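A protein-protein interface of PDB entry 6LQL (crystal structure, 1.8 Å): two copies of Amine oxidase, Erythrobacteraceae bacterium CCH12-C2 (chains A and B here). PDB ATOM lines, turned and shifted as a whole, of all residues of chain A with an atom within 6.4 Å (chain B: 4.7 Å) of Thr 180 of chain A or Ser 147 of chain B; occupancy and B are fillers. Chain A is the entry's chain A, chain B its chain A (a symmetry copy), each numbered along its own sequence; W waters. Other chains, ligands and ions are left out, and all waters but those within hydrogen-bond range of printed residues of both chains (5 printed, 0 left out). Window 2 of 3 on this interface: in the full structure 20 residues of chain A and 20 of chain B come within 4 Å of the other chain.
OE1 of Gln 152 of chain A is in hydrogen-bond range of NE2 of Gln 152 of chain B.
The side-chain amide nitrogen (NE2) of Gln 152 of chain A lies within hydrogen-bond range of the backbone carbonyl oxygen (O) of Ser 147 of chain B (3.2 Å).
O of Thr 180 of chain A lies within hydrogen-bond range of OG1 of Thr 402 of chain B, at 2.7 Å.
N of Thr 149 of chain A lies within hydrogen-bond range of OE1 of Gln 152 of chain A (2.9 Å).
The backbone NH (N) of Ser 178 of chain A sits at hydrogen-bond distance from the side-chain carboxylate (OE1) of Glu 181 of chain A, at 2.9 Å.
OG1 of Thr 180 of chain A lies within hydrogen-bond range of OG of Ser 178 of chain A (3.3 Å).
The side-chain hydroxyl (OG1) of Thr 149 of chain A sits close to the backbone NH (N) of Ala 151 of chain A.
The backbone carbonyl oxygen (O) of Gly 143 of chain B sits at hydrogen-bond distance from the side-chain hydroxyl (OG) of Ser 147 of chain B (2.8 Å).
N of Thr 149 of chain B is in hydrogen-bond range of OE1 of Gln 152 of chain B (2.9 Å).
Among the printed residues, pairs that only touch across the chains: Thr 149 of chain A with Thr 402 of chain B (3.9 Å), Gln 152 of chain A with Met 148 of chain B (3.8 Å), Thr 180 of chain A with Ser 147 of chain B (3.8 Å) and Glu 181 of chain A with Thr 402 of chain B (3.8 Å).
Of chain B, only Ser 147 and Thr 402 come within 4 Å of Thr 180 of chain A.
Of chain A, only Gln 152 (3.2 Å) and Thr 180 (3.8 Å) come within 4 Å of Ser 147 of chain B.
Of the printed residues of chain B, Gln 152 of chain A touches Ser 147 (3.2 Å), Met 148 (3.8 Å) and Gln 152 (2.8 Å).
Printed residues of chain A within 4 Å of Met 148 of chain B: Gln 152 (3.8 Å).
Val 150 of chain A touches none of the printed residues of chain B.
Glu 144 of chain B touches none of the printed residues of chain A.
The nearest residue of chain B that does not touch Thr 180 of chain A is Gly 403 of chain B (4.5 Å).
The nearest printed residue of chain A that does not touch Thr 402 of chain B is Val 182 of chain A (5.3 Å).
Of the 10 printed residues of chain B, 4 touch a printed residue of chain A.
Printed residues of chain A that touch a printed residue of chain B: Thr 149, Gln 152, Thr 180 and Glu 181.
Gln 152 of chain B touches its own counterpart, Gln 152 of chain A.
Water W5 lies within hydrogen-bond range of the side-chain carboxylate (OE2) of Glu 181 of chain A and the backbone carbonyl oxygen (O) of Gly 403 of chain B.
Water W2 lies within hydrogen-bond range of OG1 of Thr 149 of chain A and O of Ser 147 of chain B.
Water W3 bridges the side-chain hydroxyl (OG1) of Thr 402 of chain B and the backbone carbonyl oxygen (O) of Glu 181 of chain A.
Water W4 bridges OG1 of Thr 180 of chain A (2.8 Å) and OG of Ser 147 of chain B (3.3 Å).
Water W1 bridges the backbone carbonyl oxygen (O) of Thr 402 of chain B (2.8 Å) and the backbone carbonyl oxygen (O) of Glu 181 of chain A (2.9 Å).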
ATOM      1  N   THR A 149      -6.154 -12.357  19.781  1.00  0.00           N
ATOM      2  CA  THR A 149      -5.037 -12.047  18.901  1.00  0.00           C
ATOM      3  C   THR A 149      -4.589 -10.599  19.073  1.00  0.00           C
ATOM      4  O   THR A 149      -5.292  -9.758  19.660  1.00  0.00           O
ATOM      5  CB  THR A 149      -5.414 -12.264  17.442  1.00  0.00           C
ATOM      6  OG1 THR A 149      -6.394 -11.274  17.081  1.00  0.00           O
ATOM      7  CG2 THR A 149      -5.977 -13.668  17.204  1.00  0.00           C
ATOM      8  N   VAL A 150      -3.400 -10.305  18.535  1.00  0.00           N
ATOM      9  CA  VAL A 150      -2.932  -8.922  18.528  1.00  0.00           C
ATOM     10  C   VAL A 150      -3.884  -8.054  17.709  1.00  0.00           C
ATOM     11  O   VAL A 150      -4.191  -6.915  18.086  1.00  0.00           O
ATOM     12  CB  VAL A 150      -1.487  -8.832  18.000  1.00  0.00           C
ATOM     13  CG1 VAL A 150      -1.018  -7.381  17.994  1.00  0.00           C
ATOM     14  CG2 VAL A 150      -0.529  -9.680  18.847  1.00  0.00           C
ATOM     15  N   ALA A 151      -4.381  -8.582  16.587  1.00  0.00           N
ATOM     16  CA  ALA A 151      -5.328  -7.827  15.773  1.00  0.00           C
ATOM     17  C   ALA A 151      -6.565  -7.431  16.577  1.00  0.00           C
ATOM     18  O   ALA A 151      -7.063  -6.308  16.460  1.00  0.00           O
ATOM     19  CB  ALA A 151      -5.733  -8.644  14.554  1.00  0.00           C
ATOM     20  N   GLN A 152      -7.077  -8.342  17.396  1.00  0.00           N
ATOM     21  CA  GLN A 152      -8.252  -8.003  18.194  1.00  0.00           C
ATOM     22  C   GLN A 152      -7.931  -6.937  19.243  1.00  0.00           C
ATOM     23  O   GLN A 152      -8.749  -6.036  19.503  1.00  0.00           O
ATOM     24  CB  GLN A 152      -8.806  -9.283  18.819  1.00  0.00           C
ATOM     25  CG  GLN A 152      -9.377 -10.209  17.759  1.00  0.00           C
ATOM     26  CD  GLN A 152      -9.596 -11.633  18.224  1.00  0.00           C
ATOM     27  OE1 GLN A 152      -8.967 -12.098  19.184  1.00  0.00           O
ATOM     28  NE2 GLN A 152     -10.493 -12.345  17.529  1.00  0.00           N
ATOM     29  N   ALA A 177       4.857 -12.811  11.732  1.00  0.00           N
ATOM     30  CA  ALA A 177       3.533 -13.405  11.609  1.00  0.00           C
ATOM     31  C   ALA A 177       2.493 -12.301  11.681  1.00  0.00           C
ATOM     32  O   ALA A 177       2.757 -11.211  12.191  1.00  0.00           O
ATOM     33  CB  ALA A 177       3.255 -14.440  12.711  1.00  0.00           C
ATOM     34  N   SER A 178       1.308 -12.608  11.171  1.00  0.00           N
ATOM     35  CA  SER A 178       0.234 -11.624  11.121  1.00  0.00           C
ATOM     36  C   SER A 178      -0.309 -11.321  12.519  1.00  0.00           C
ATOM     37  O   SER A 178      -0.295 -12.166  13.420  1.00  0.00           O
ATOM     38  CB  SER A 178      -0.891 -12.130  10.222  1.00  0.00           C
ATOM     39  OG  SER A 178      -1.923 -11.163  10.083  1.00  0.00           O
ATOM     40  N   THR A 179      -0.822 -10.096  12.689  1.00  0.00           N
ATOM     41  CA  THR A 179      -1.518  -9.779  13.934  1.00  0.00           C
ATOM     42  C   THR A 179      -2.722 -10.687  14.167  1.00  0.00           C
ATOM     43  O   THR A 179      -3.143 -10.855  15.318  1.00  0.00           O
ATOM     44  CB  THR A 179      -1.963  -8.305  13.946  1.00  0.00           C
ATOM     45  OG1 THR A 179      -2.737  -8.021  12.769  1.00  0.00           O
ATOM     46  CG2 THR A 179      -0.750  -7.379  13.998  1.00  0.00           C
ATOM     47  N   THR A 180      -3.305 -11.262  13.111  1.00  0.00           N
ATOM     48  CA  THR A 180      -4.419 -12.179  13.308  1.00  0.00           C
ATOM     49  C   THR A 180      -3.968 -13.581  13.688  1.00  0.00           C
ATOM     50  O   THR A 180      -4.818 -14.421  14.005  1.00  0.00           O
ATOM     51  CB  THR A 180      -5.286 -12.279  12.053  1.00  0.00           C
ATOM     52  OG1 THR A 180      -4.538 -12.925  11.009  1.00  0.00           O
ATOM     53  CG2 THR A 180      -5.751 -10.888  11.605  1.00  0.00           C
ATOM     54  N   GLU A 181      -2.661 -13.842  13.655  1.00  0.00           N
ATOM     55  CA  GLU A 181      -2.118 -15.167  13.936  1.00  0.00           C
ATOM     56  C   GLU A 181      -1.493 -15.286  15.316  1.00  0.00           C
ATOM     57  O   GLU A 181      -1.477 -16.388  15.877  1.00  0.00           O
ATOM     58  CB  GLU A 181      -1.053 -15.526  12.890  1.00  0.00           C
ATOM     59  CG  GLU A 181      -1.628 -15.681  11.496  1.00  0.00           C
ATOM     60  CD  GLU A 181      -0.567 -15.610  10.370  1.00  0.00           C
ATOM     61  OE1 GLU A 181       0.635 -15.405  10.652  1.00  0.00           O
ATOM     62  OE2 GLU A 181      -0.953 -15.768   9.188  1.00  0.00           O
ATOM     63  N   VAL A 182      -1.006 -14.181  15.879  1.00  0.00           N
ATOM     64  CA  VAL A 182      -0.205 -14.183  17.101  1.00  0.00           C
ATOM     65  C   VAL A 182      -1.099 -13.890  18.297  1.00  0.00           C
ATOM     66  O   VAL A 182      -1.901 -12.944  18.275  1.00  0.00           O
ATOM     67  CB  VAL A 182       0.931 -13.150  17.023  1.00  0.00           C
ATOM     68  CG1 VAL A 182       1.772 -13.207  18.302  1.00  0.00           C
ATOM     69  CG2 VAL A 182       1.831 -13.394  15.787  1.00  0.00           C
ATOM     70  N   GLY B 143     -12.095 -14.591   5.596  1.00  0.00           N
ATOM     71  CA  GLY B 143     -11.073 -13.812   6.286  1.00  0.00           C
ATOM     72  C   GLY B 143     -11.494 -13.414   7.693  1.00  0.00           C
ATOM     73  O   GLY B 143     -10.750 -13.599   8.676  1.00  0.00           O
ATOM     74  N   GLU B 144     -12.722 -12.911   7.822  1.00  0.00           N
ATOM     75  CA  GLU B 144     -13.203 -12.498   9.135  1.00  0.00           C
ATOM     76  C   GLU B 144     -13.415 -13.699  10.057  1.00  0.00           C
ATOM     77  O   GLU B 144     -13.062 -13.658  11.242  1.00  0.00           O
ATOM     78  CB  GLU B 144     -14.492 -11.691   8.979  1.00  0.00           C
ATOM     79  CG  GLU B 144     -14.894 -10.966  10.238  1.00  0.00           C
ATOM     80  CD  GLU B 144     -16.064 -10.021  10.024  1.00  0.00           C
ATOM     81  OE1 GLU B 144     -16.188  -9.467   8.910  1.00  0.00           O
ATOM     82  OE2 GLU B 144     -16.865  -9.843  10.970  1.00  0.00           O
ATOM     83  N   LEU B 145     -14.031 -14.762   9.545  1.00  0.00           N
ATOM     84  CA  LEU B 145     -14.275 -15.930  10.383  1.00  0.00           C
ATOM     85  C   LEU B 145     -12.964 -16.566  10.826  1.00  0.00           C
ATOM     86  O   LEU B 145     -12.866 -17.089  11.943  1.00  0.00           O
ATOM     87  CB  LEU B 145     -15.143 -16.945   9.630  1.00  0.00           C
ATOM     88  CG  LEU B 145     -16.614 -16.556   9.498  1.00  0.00           C
ATOM     89  CD1 LEU B 145     -17.271 -17.359   8.359  1.00  0.00           C
ATOM     90  CD2 LEU B 145     -17.356 -16.761  10.801  1.00  0.00           C
ATOM     91  N   ASP B 146     -11.940 -16.494   9.979  1.00  0.00           N
ATOM     92  CA  ASP B 146     -10.651 -17.128  10.243  1.00  0.00           C
ATOM     93  C   ASP B 146      -9.786 -16.281  11.154  1.00  0.00           C
ATOM     94  O   ASP B 146      -8.696 -16.725  11.552  1.00  0.00           O
ATOM     95  CB  ASP B 146      -9.914 -17.379   8.915  1.00  0.00           C
ATOM     96  CG  ASP B 146      -8.838 -18.460   9.026  1.00  0.00           C
ATOM     97  OD1 ASP B 146      -9.068 -19.432   9.766  1.00  0.00           O
ATOM     98  OD2 ASP B 146      -7.796 -18.345   8.340  1.00  0.00           O
ATOM     99  N   SER B 147     -10.216 -15.051  11.436  1.00  0.00           N
ATOM    100  CA  SER B 147      -9.513 -14.205  12.391  1.00  0.00           C
ATOM    101  C   SER B 147     -10.052 -14.290  13.823  1.00  0.00           C
ATOM    102  O   SER B 147      -9.544 -13.589  14.704  1.00  0.00           O
ATOM    103  CB  SER B 147      -9.563 -12.759  11.907  1.00  0.00           C
ATOM    104  OG  SER B 147      -9.011 -12.673  10.604  1.00  0.00           O
ATOM    105  N   MET B 148     -11.042 -15.136  14.087  1.00  0.00           N
ATOM    106  CA  MET B 148     -11.588 -15.306  15.424  1.00  0.00           C
ATOM    107  C   MET B 148     -11.615 -16.782  15.801  1.00  0.00           C
ATOM    108  O   MET B 148     -11.566 -17.664  14.938  1.00  0.00           O
ATOM    109  CB  MET B 148     -13.006 -14.740  15.512  1.00  0.00           C
ATOM    110  CG  MET B 148     -13.994 -15.578  14.746  1.00  0.00           C
ATOM    111  SD  MET B 148     -15.608 -14.784  14.585  1.00  0.00           S
ATOM    112  CE  MET B 148     -16.110 -14.645  16.274  1.00  0.00           C
ATOM    113  N   THR B 149     -11.702 -17.044  17.105  1.00  0.00           N
ATOM    114  CA  THR B 149     -11.747 -18.408  17.609  1.00  0.00           C
ATOM    115  C   THR B 149     -13.187 -18.880  17.784  1.00  0.00           C
ATOM    116  O   THR B 149     -14.145 -18.087  17.778  1.00  0.00           O
ATOM    117  CB  THR B 149     -11.037 -18.518  18.952  1.00  0.00           C
ATOM    118  OG1 THR B 149     -11.807 -17.787  19.925  1.00  0.00           O
ATOM    119  CG2 THR B 149      -9.612 -17.962  18.888  1.00  0.00           C
ATOM    120  N   GLN B 152     -14.642 -17.257  20.842  1.00  0.00           N
ATOM    121  CA  GLN B 152     -15.178 -15.914  20.641  1.00  0.00           C
ATOM    122  C   GLN B 152     -16.546 -15.949  19.960  1.00  0.00           C
ATOM    123  O   GLN B 152     -17.446 -15.160  20.301  1.00  0.00           O
ATOM    124  CB  GLN B 152     -14.159 -15.092  19.854  1.00  0.00           C
ATOM    125  CG  GLN B 152     -12.907 -14.835  20.676  1.00  0.00           C
ATOM    126  CD  GLN B 152     -11.713 -14.371  19.870  1.00  0.00           C
ATOM    127  OE1 GLN B 152     -11.624 -14.612  18.659  1.00  0.00           O
ATOM    128  NE2 GLN B 152     -10.772 -13.702  20.550  1.00  0.00           N
ATOM    129  N   THR B 402      -6.180 -19.505  14.146  1.00  0.00           N
ATOM    130  CA  THR B 402      -6.572 -18.349  13.346  1.00  0.00           C
ATOM    131  C   THR B 402      -5.559 -18.063  12.245  1.00  0.00           C
ATOM    132  O   THR B 402      -4.343 -18.140  12.456  1.00  0.00           O
ATOM    133  CB  THR B 402      -6.724 -17.102  14.221  1.00  0.00           C
ATOM    134  OG1 THR B 402      -5.524 -16.871  14.975  1.00  0.00           O
ATOM    135  CG2 THR B 402      -7.909 -17.270  15.170  1.00  0.00           C
ATOM    136  N   GLY B 403      -6.081 -17.711  11.067  1.00  0.00           N
ATOM    137  CA  GLY B 403      -5.282 -17.210   9.981  1.00  0.00           C
ATOM    138  C   GLY B 403      -4.813 -18.239   8.978  1.00  0.00           C
ATOM    139  O   GLY B 403      -4.377 -17.846   7.888  1.00  0.00           O
HETATM  140  O   HOH W   1      -2.177 -18.637  14.229  1.00  0.00           O
HETATM  141  O   HOH W   2      -7.689 -11.581  14.789  1.00  0.00           O
HETATM  142  O   HOH W   3      -3.850 -17.280  17.163  1.00  0.00           O
HETATM  143  O   HOH W   4      -6.383 -13.895   9.109  1.00  0.00           O
HETATM  144  O   HOH W   5      -3.133 -15.071   7.908  1.00  0.00           O
